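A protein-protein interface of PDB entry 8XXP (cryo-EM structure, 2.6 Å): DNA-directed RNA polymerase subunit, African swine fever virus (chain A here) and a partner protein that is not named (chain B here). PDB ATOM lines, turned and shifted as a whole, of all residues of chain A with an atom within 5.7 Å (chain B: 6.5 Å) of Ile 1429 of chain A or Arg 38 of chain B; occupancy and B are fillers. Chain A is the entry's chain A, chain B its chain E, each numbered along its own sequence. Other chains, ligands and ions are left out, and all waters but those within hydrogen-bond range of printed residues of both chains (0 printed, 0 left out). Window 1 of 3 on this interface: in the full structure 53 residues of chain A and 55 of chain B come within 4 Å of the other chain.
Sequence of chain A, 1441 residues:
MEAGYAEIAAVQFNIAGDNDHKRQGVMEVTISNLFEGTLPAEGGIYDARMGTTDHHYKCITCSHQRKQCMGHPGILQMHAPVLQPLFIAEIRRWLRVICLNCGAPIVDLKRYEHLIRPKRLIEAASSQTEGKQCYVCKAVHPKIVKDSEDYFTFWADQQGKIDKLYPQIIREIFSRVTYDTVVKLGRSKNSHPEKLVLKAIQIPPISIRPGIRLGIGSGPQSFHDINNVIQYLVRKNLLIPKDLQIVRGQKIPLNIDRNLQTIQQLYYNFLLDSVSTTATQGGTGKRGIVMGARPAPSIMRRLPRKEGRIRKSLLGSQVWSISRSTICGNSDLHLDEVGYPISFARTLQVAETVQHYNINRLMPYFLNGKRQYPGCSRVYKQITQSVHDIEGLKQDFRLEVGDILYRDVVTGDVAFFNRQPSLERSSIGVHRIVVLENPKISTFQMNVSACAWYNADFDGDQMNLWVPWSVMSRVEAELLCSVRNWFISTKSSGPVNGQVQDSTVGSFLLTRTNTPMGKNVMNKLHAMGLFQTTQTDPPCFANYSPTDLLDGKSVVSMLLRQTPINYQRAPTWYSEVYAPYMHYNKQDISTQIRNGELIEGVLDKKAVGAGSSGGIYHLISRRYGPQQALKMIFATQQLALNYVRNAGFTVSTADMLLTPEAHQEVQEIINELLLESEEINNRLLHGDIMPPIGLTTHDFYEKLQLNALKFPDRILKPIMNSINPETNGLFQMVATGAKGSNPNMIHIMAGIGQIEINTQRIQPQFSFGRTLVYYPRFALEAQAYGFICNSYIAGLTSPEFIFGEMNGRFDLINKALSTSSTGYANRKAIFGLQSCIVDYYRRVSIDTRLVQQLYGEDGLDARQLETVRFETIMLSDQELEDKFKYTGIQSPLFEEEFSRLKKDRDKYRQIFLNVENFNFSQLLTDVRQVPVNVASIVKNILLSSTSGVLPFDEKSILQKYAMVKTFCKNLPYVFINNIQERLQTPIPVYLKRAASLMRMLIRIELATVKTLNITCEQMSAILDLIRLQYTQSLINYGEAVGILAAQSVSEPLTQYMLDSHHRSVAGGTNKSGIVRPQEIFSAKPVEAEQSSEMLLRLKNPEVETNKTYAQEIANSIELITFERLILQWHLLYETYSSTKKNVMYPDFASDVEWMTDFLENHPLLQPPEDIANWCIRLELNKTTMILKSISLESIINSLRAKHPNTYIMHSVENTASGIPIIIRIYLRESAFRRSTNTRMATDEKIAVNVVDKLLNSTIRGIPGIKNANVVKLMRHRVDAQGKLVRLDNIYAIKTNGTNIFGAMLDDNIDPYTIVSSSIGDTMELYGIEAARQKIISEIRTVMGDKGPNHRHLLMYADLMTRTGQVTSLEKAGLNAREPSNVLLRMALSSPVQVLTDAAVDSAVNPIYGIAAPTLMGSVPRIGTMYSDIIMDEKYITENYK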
ATOM      1  N   MET A 472      -1.736 -18.572 -29.335  1.00  0.00           N
ATOM      2  CA  MET A 472      -2.554 -17.798 -28.408  1.00  0.00           C
ATOM      3  C   MET A 472      -3.925 -18.427 -28.223  1.00  0.00           C
ATOM      4  O   MET A 472      -4.434 -18.503 -27.101  1.00  0.00           O
ATOM      5  CB  MET A 472      -2.702 -16.366 -28.907  1.00  0.00           C
ATOM      6  CG  MET A 472      -1.420 -15.577 -28.987  1.00  0.00           C
ATOM      7  SD  MET A 472      -1.724 -13.850 -28.617  1.00  0.00           S
ATOM      8  CE  MET A 472      -0.157 -13.361 -27.943  1.00  0.00           C
ATOM      9  N   THR A1424      -9.727 -11.609 -21.647  1.00  0.00           N
ATOM     10  CA  THR A1424      -8.309 -11.803 -21.927  1.00  0.00           C
ATOM     11  C   THR A1424      -7.669 -10.537 -22.478  1.00  0.00           C
ATOM     12  O   THR A1424      -6.457 -10.351 -22.341  1.00  0.00           O
ATOM     13  CB  THR A1424      -8.090 -12.974 -22.881  1.00  0.00           C
ATOM     14  OG1 THR A1424      -9.038 -12.913 -23.947  1.00  0.00           O
ATOM     15  CG2 THR A1424      -8.233 -14.287 -22.148  1.00  0.00           C
ATOM     16  N   MET A1425      -8.455  -9.651 -23.081  1.00  0.00           N
ATOM     17  CA  MET A1425      -7.954  -8.365 -23.538  1.00  0.00           C
ATOM     18  C   MET A1425      -8.203  -7.244 -22.547  1.00  0.00           C
ATOM     19  O   MET A1425      -7.899  -6.091 -22.857  1.00  0.00           O
ATOM     20  CB  MET A1425      -8.580  -7.982 -24.878  1.00  0.00           C
ATOM     21  CG  MET A1425      -8.696  -9.092 -25.876  1.00  0.00           C
ATOM     22  SD  MET A1425      -7.258  -9.351 -26.916  1.00  0.00           S
ATOM     23  CE  MET A1425      -6.271 -10.421 -25.892  1.00  0.00           C
ATOM     24  N   SER A1427      -6.870  -6.565 -19.492  1.00  0.00           N
ATOM     25  CA  SER A1427      -5.652  -6.025 -18.913  1.00  0.00           C
ATOM     26  C   SER A1427      -4.564  -5.983 -19.970  1.00  0.00           C
ATOM     27  O   SER A1427      -4.405  -6.932 -20.743  1.00  0.00           O
ATOM     28  CB  SER A1427      -5.189  -6.860 -17.720  1.00  0.00           C
ATOM     29  OG  SER A1427      -6.150  -6.847 -16.683  1.00  0.00           O
ATOM     30  N   ASP A1428      -3.828  -4.882 -20.009  1.00  0.00           N
ATOM     31  CA  ASP A1428      -2.703  -4.760 -20.916  1.00  0.00           C
ATOM     32  C   ASP A1428      -1.490  -5.489 -20.362  1.00  0.00           C
ATOM     33  O   ASP A1428      -1.218  -5.452 -19.161  1.00  0.00           O
ATOM     34  CB  ASP A1428      -2.364  -3.293 -21.156  1.00  0.00           C
ATOM     35  CG  ASP A1428      -3.131  -2.705 -22.320  1.00  0.00           C
ATOM     36  OD1 ASP A1428      -2.592  -2.701 -23.447  1.00  0.00           O
ATOM     37  OD2 ASP A1428      -4.274  -2.246 -22.109  1.00  0.00           O
ATOM     38  N   ILE A1429      -0.763  -6.155 -21.248  1.00  0.00           N
ATOM     39  CA  ILE A1429       0.493  -6.808 -20.914  1.00  0.00           C
ATOM     40  C   ILE A1429       1.621  -5.939 -21.445  1.00  0.00           C
ATOM     41  O   ILE A1429       1.594  -5.521 -22.606  1.00  0.00           O
ATOM     42  CB  ILE A1429       0.565  -8.223 -21.512  1.00  0.00           C
ATOM     43  CG1 ILE A1429      -0.686  -9.029 -21.163  1.00  0.00           C
ATOM     44  CG2 ILE A1429       1.816  -8.931 -21.040  1.00  0.00           C
ATOM     45  CD1 ILE A1429      -0.998  -9.106 -19.689  1.00  0.00           C
ATOM     46  N   ILE A1430       2.595  -5.644 -20.596  1.00  0.00           N
ATOM     47  CA  ILE A1430       3.780  -4.903 -20.995  1.00  0.00           C
ATOM     48  C   ILE A1430       4.998  -5.760 -20.695  1.00  0.00           C
ATOM     49  O   ILE A1430       5.010  -6.522 -19.726  1.00  0.00           O
ATOM     50  CB  ILE A1430       3.880  -3.532 -20.295  1.00  0.00           C
ATOM     51  CG1 ILE A1430       4.092  -3.701 -18.797  1.00  0.00           C
ATOM     52  CG2 ILE A1430       2.639  -2.717 -20.555  1.00  0.00           C
ATOM     53  CD1 ILE A1430       4.146  -2.410 -18.050  1.00  0.00           C
ATOM     54  N   MET A1431       6.006  -5.659 -21.548  1.00  0.00           N
ATOM     55  CA  MET A1431       7.196  -6.474 -21.379  1.00  0.00           C
ATOM     56  C   MET A1431       7.984  -5.989 -20.170  1.00  0.00           C
ATOM     57  O   MET A1431       8.165  -4.786 -19.970  1.00  0.00           O
ATOM     58  CB  MET A1431       8.056  -6.408 -22.638  1.00  0.00           C
ATOM     59  CG  MET A1431       7.384  -6.972 -23.876  1.00  0.00           C
ATOM     60  SD  MET A1431       7.252  -8.759 -23.993  1.00  0.00           S
ATOM     61  CE  MET A1431       8.822  -9.273 -23.342  1.00  0.00           C
ATOM     62  N   THR B  33      -8.157 -15.398 -13.934  1.00  0.00           N
ATOM     63  CA  THR B  33      -7.954 -16.435 -14.937  1.00  0.00           C
ATOM     64  C   THR B  33      -7.740 -15.816 -16.307  1.00  0.00           C
ATOM     65  O   THR B  33      -6.972 -16.337 -17.121  1.00  0.00           O
ATOM     66  CB  THR B  33      -9.134 -17.400 -14.965  1.00  0.00           C
ATOM     67  OG1 THR B  33     -10.348 -16.673 -15.177  1.00  0.00           O
ATOM     68  CG2 THR B  33      -9.225 -18.150 -13.660  1.00  0.00           C
ATOM     69  N   PHE B  34      -8.403 -14.692 -16.571  1.00  0.00           N
ATOM     70  CA  PHE B  34      -8.194 -13.973 -17.820  1.00  0.00           C
ATOM     71  C   PHE B  34      -6.762 -13.476 -17.935  1.00  0.00           C
ATOM     72  O   PHE B  34      -6.120 -13.637 -18.975  1.00  0.00           O
ATOM     73  CB  PHE B  34      -9.160 -12.801 -17.906  1.00  0.00           C
ATOM     74  CG  PHE B  34     -10.590 -13.202 -18.022  1.00  0.00           C
ATOM     75  CD1 PHE B  34     -10.956 -14.277 -18.798  1.00  0.00           C
ATOM     76  CD2 PHE B  34     -11.573 -12.486 -17.370  1.00  0.00           C
ATOM     77  CE1 PHE B  34     -12.270 -14.636 -18.911  1.00  0.00           C
ATOM     78  CE2 PHE B  34     -12.881 -12.839 -17.485  1.00  0.00           C
ATOM     79  CZ  PHE B  34     -13.234 -13.916 -18.255  1.00  0.00           C
ATOM     80  N   GLU B  35      -6.248 -12.858 -16.873  1.00  0.00           N
ATOM     81  CA  GLU B  35      -4.909 -12.284 -16.930  1.00  0.00           C
ATOM     82  C   GLU B  35      -3.846 -13.367 -16.998  1.00  0.00           C
ATOM     83  O   GLU B  35      -2.864 -13.227 -17.731  1.00  0.00           O
ATOM     84  CB  GLU B  35      -4.676 -11.370 -15.730  1.00  0.00           C
ATOM     85  CG  GLU B  35      -5.390 -10.044 -15.850  1.00  0.00           C
ATOM     86  CD  GLU B  35      -5.450  -9.274 -14.553  1.00  0.00           C
ATOM     87  OE1 GLU B  35      -5.268  -9.880 -13.481  1.00  0.00           O
ATOM     88  OE2 GLU B  35      -5.699  -8.055 -14.610  1.00  0.00           O
ATOM     89  N   ALA B  36      -4.021 -14.452 -16.244  1.00  0.00           N
ATOM     90  CA  ALA B  36      -3.083 -15.566 -16.325  1.00  0.00           C
ATOM     91  C   ALA B  36      -3.106 -16.209 -17.705  1.00  0.00           C
ATOM     92  O   ALA B  36      -2.051 -16.527 -18.267  1.00  0.00           O
ATOM     93  CB  ALA B  36      -3.399 -16.595 -15.245  1.00  0.00           C
ATOM     94  N   THR B  37      -4.300 -16.409 -18.265  1.00  0.00           N
ATOM     95  CA  THR B  37      -4.412 -16.973 -19.605  1.00  0.00           C
ATOM     96  C   THR B  37      -3.746 -16.074 -20.636  1.00  0.00           C
ATOM     97  O   THR B  37      -3.030 -16.554 -21.518  1.00  0.00           O
ATOM     98  CB  THR B  37      -5.883 -17.185 -19.957  1.00  0.00           C
ATOM     99  OG1 THR B  37      -6.474 -18.091 -19.020  1.00  0.00           O
ATOM    100  CG2 THR B  37      -6.026 -17.749 -21.351  1.00  0.00           C
ATOM    101  N   ARG B  38      -3.967 -14.765 -20.537  1.00  0.00           N
ATOM    102  CA  ARG B  38      -3.347 -13.832 -21.466  1.00  0.00           C
ATOM    103  C   ARG B  38      -1.833 -13.825 -21.318  1.00  0.00           C
ATOM    104  O   ARG B  38      -1.109 -13.746 -22.314  1.00  0.00           O
ATOM    105  CB  ARG B  38      -3.919 -12.434 -21.246  1.00  0.00           C
ATOM    106  CG  ARG B  38      -3.239 -11.341 -22.033  1.00  0.00           C
ATOM    107  CD  ARG B  38      -3.477 -11.476 -23.514  1.00  0.00           C
ATOM    108  NE  ARG B  38      -2.991 -10.306 -24.229  1.00  0.00           N
ATOM    109  CZ  ARG B  38      -2.822 -10.243 -25.541  1.00  0.00           C
ATOM    110  NH1 ARG B  38      -3.088 -11.276 -26.320  1.00  0.00           N
ATOM    111  NH2 ARG B  38      -2.381  -9.115 -26.084  1.00  0.00           N
ATOM    112  N   LEU B  39      -1.333 -13.892 -20.084  1.00  0.00           N
ATOM    113  CA  LEU B  39       0.108 -13.922 -19.870  1.00  0.00           C
ATOM    114  C   LEU B  39       0.725 -15.161 -20.490  1.00  0.00           C
ATOM    115  O   LEU B  39       1.758 -15.085 -21.163  1.00  0.00           O
ATOM    116  CB  LEU B  39       0.419 -13.873 -18.379  1.00  0.00           C
ATOM    117  CG  LEU B  39       0.251 -12.536 -17.677  1.00  0.00           C
ATOM    118  CD1 LEU B  39       0.278 -12.766 -16.194  1.00  0.00           C
ATOM    119  CD2 LEU B  39       1.337 -11.579 -18.094  1.00  0.00           C
ATOM    120  N   VAL B  40       0.099 -16.317 -20.276  1.00  0.00           N
ATOM    121  CA  VAL B  40       0.624 -17.548 -20.853  1.00  0.00           C
ATOM    122  C   VAL B  40       0.558 -17.496 -22.372  1.00  0.00           C
ATOM    123  O   VAL B  40       1.494 -17.916 -23.054  1.00  0.00           O
ATOM    124  CB  VAL B  40      -0.116 -18.771 -20.284  1.00  0.00           C
ATOM    125  CG1 VAL B  40       0.397 -20.042 -20.917  1.00  0.00           C
ATOM    126  CG2 VAL B  40       0.078 -18.842 -18.794  1.00  0.00           C
ATOM    127  N   ALA B  41      -0.534 -16.969 -22.928  1.00  0.00           N
ATOM    128  CA  ALA B  41      -0.670 -16.902 -24.380  1.00  0.00           C
ATOM    129  C   ALA B  41       0.371 -15.982 -24.999  1.00  0.00           C
ATOM    130  O   ALA B  41       0.984 -16.323 -26.016  1.00  0.00           O
ATOM    131  CB  ALA B  41      -2.075 -16.440 -24.751  1.00  0.00           C
ATOM    132  N   VAL B  42       0.588 -14.812 -24.400  1.00  0.00           N
ATOM    133  CA  VAL B  42       1.593 -13.885 -24.909  1.00  0.00           C
ATOM    134  C   VAL B  42       2.980 -14.502 -24.812  1.00  0.00           C
ATOM    135  O   VAL B  42       3.772 -14.448 -25.761  1.00  0.00           O
ATOM    136  CB  VAL B  42       1.518 -12.547 -24.155  1.00  0.00           C
ATOM    137  CG1 VAL B  42       2.716 -11.688 -24.479  1.00  0.00           C
ATOM    138  CG2 VAL B  42       0.250 -11.824 -24.510  1.00  0.00           C
ATOM    139  N   ARG B  43       3.296 -15.106 -23.664  1.00  0.00           N
ATOM    140  CA  ARG B  43       4.616 -15.693 -23.494  1.00  0.00           C
ATOM    141  C   ARG B  43       4.841 -16.837 -24.468  1.00  0.00           C
ATOM    142  O   ARG B  43       5.936 -16.985 -25.018  1.00  0.00           O
ATOM    143  CB  ARG B  43       4.797 -16.173 -22.058  1.00  0.00           C
ATOM    144  CG  ARG B  43       6.190 -16.669 -21.770  1.00  0.00           C
ATOM    145  CD  ARG B  43       7.206 -15.596 -22.062  1.00  0.00           C
ATOM    146  NE  ARG B  43       8.574 -16.076 -21.912  1.00  0.00           N
ATOM    147  CZ  ARG B  43       9.611 -15.585 -22.575  1.00  0.00           C
ATOM    148  NH1 ARG B  43       9.471 -14.598 -23.443  1.00  0.00           N
ATOM    149  NH2 ARG B  43      10.819 -16.092 -22.358  1.00  0.00           N
ATOM    150  N   LEU B  77       6.993 -10.804 -18.054  1.00  0.00           N
ATOM    151  CA  LEU B  77       5.912  -9.921 -18.449  1.00  0.00           C
ATOM    152  C   LEU B  77       5.401  -9.183 -17.225  1.00  0.00           C
ATOM    153  O   LEU B  77       5.676  -9.561 -16.087  1.00  0.00           O
ATOM    154  CB  LEU B  77       4.769 -10.696 -19.118  1.00  0.00           C
ATOM    155  CG  LEU B  77       5.126 -11.516 -20.358  1.00  0.00           C
ATOM    156  CD1 LEU B  77       3.920 -12.268 -20.873  1.00  0.00           C
ATOM    157  CD2 LEU B  77       5.688 -10.624 -21.437  1.00  0.00           C
ATOM    158  N   LEU B  78       4.665  -8.109 -17.477  1.00  0.00           N
ATOM    159  CA  LEU B  78       3.997  -7.358 -16.430  1.00  0.00           C
ATOM    160  C   LEU B  78       2.544  -7.158 -16.820  1.00  0.00           C
ATOM    161  O   LEU B  78       2.206  -7.116 -18.003  1.00  0.00           O
ATOM    162  CB  LEU B  78       4.653  -6.003 -16.195  1.00  0.00           C
ATOM    163  CG  LEU B  78       6.078  -5.996 -15.663  1.00  0.00           C
ATOM    164  CD1 LEU B  78       6.625  -4.600 -15.726  1.00  0.00           C
ATOM    165  CD2 LEU B  78       6.108  -6.523 -14.250  1.00  0.00           C
ATOM    166  N   VAL B  79       1.685  -7.042 -15.818  1.00  0.00           N
ATOM    167  CA  VAL B  79       0.268  -6.784 -16.028  1.00  0.00           C
ATOM    168  C   VAL B  79       0.010  -5.333 -15.672  1.00  0.00           C
ATOM    169  O   VAL B  79       0.149  -4.937 -14.510  1.00  0.00           O
ATOM    170  CB  VAL B  79      -0.614  -7.722 -15.195  1.00  0.00           C
ATOM    171  CG1 VAL B  79      -2.073  -7.379 -15.394  1.00  0.00           C
ATOM    172  CG2 VAL B  79      -0.352  -9.159 -15.576  1.00  0.00           C
ATOM    173  N   MET B  80      -0.364  -4.539 -16.663  1.00  0.00           N
ATOM    174  CA  MET B  80      -0.704  -3.143 -16.447  1.00  0.00           C
ATOM    175  C   MET B  80      -2.219  -3.017 -16.460  1.00  0.00           C
ATOM    176  O   MET B  80      -2.864  -3.346 -17.460  1.00  0.00           O
ATOM    177  CB  MET B  80      -0.069  -2.251 -17.511  1.00  0.00           C
ATOM    178  CG  MET B  80      -0.846  -0.995 -17.796  1.00  0.00           C
ATOM    179  SD  MET B  80       0.006   0.104 -18.928  1.00  0.00           S
ATOM    180  CE  MET B  80      -1.299   0.384 -20.114  1.00  0.00           C
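Of the 15 printed residues of chain B, 10 touch a printed residue of chain A. Hydrophobic or aromatic side chains of chain B that line the printed part of chain A: Phe 34, Leu 39, Ala 41, Val 42, Leu 77, Leu 78, Val 79 and Met 80. Hydrophobic or aromatic side chains of chain A that line the printed part of chain B: Met 472, Met 1425, Ile 1429, Ile 1430 and Met 1431. Among the printed residues, 18 pairs touch across the chains. Among the printed residues, no Asp or Glu carboxylate lies within 4 Å of a Lys or Arg side-chain nitrogen of the other chain.
Of chain B, only Arg 38 (3.6 Å), Leu 39 (3.8 Å), Leu 77 (3.9 Å) and Leu 78 (3.4 Å) come within 4 Å of Ile 1429 of chain A. Printed residues of chain A within 4 Å of Arg 38 of chain B: Met 472, Thr 1424, Met 1425 and Ile 1429. Printed residues of chain A within 4 Å of Leu 39 of chain B: Ile 1429 (3.8 Å). Of the printed residues of chain A, Met 80 of chain B touches Asp 1428. Printed residues of chain A within 4 Å of Leu 78 of chain B: Asp 1428 (3.98 Å), Ile 1429 (3.4 Å) and Ile 1430 (2.8 Å). Of the printed residues of chain B, Ser 1427 of chain A touches Glu 35 and Val 79. Of the printed residues of chain A, Ala 41 of chain B touches Met 472. Ala 36 of chain B touches none of the printed residues of chain A. The nearest residue of chain A that does not touch Arg 38 of chain B is Ser 1427 of chain A (4.7 Å). The nearest printed residue of chain B that does not touch Thr 1424 of chain A is Thr 37 of chain B (4.2 Å).
The guanidinium group of Arg 38 of chain B sits at hydrogen-bond distance from the side-chain sulfur of Met 472 of chain A (3.7 Å). The backbone carbonyl oxygen of Asp 1428 of chain A lies within hydrogen-bond range of the backbone NH of Met 80 of chain B (2.8 Å). The backbone carbonyl oxygen (O) of Ile 1430 of chain A sits at hydrogen-bond distance from the backbone NH (N) of Leu 78 of chain B, at 2.8 Å. The side-chain hydroxyl (OG) of Ser 1427 of chain A lies within hydrogen-bond range of the side-chain carboxylate (OE2) of Glu 35 of chain B.
Among the printed residues, pairs that only touch across the chains: Met 472 of chain A with Ala 41 of chain B, Met 472 of chain A with Val 42 of chain B, Thr 1424 of chain A with Phe 34 of chain B, Thr 1424 of chain A with Arg 38 of chain B, Met 1425 of chain A with Arg 38 of chain B, Ser 1427 of chain A with Val 79 of chain B, Asp 1428 of chain A with Leu 78 of chain B, Asp 1428 of chain A with Val 79 of chain B, Ile 1429 of chain A with Arg 38 of chain B, Ile 1429 of chain A with Leu 39 of chain B, Ile 1429 of chain A with Leu 77 of chain B, Ile 1429 of chain A with Leu 78 of chain B, Ile 1430 of chain A with Leu 77 of chain B and Met 1431 of chain A with Leu 77 of chain B.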
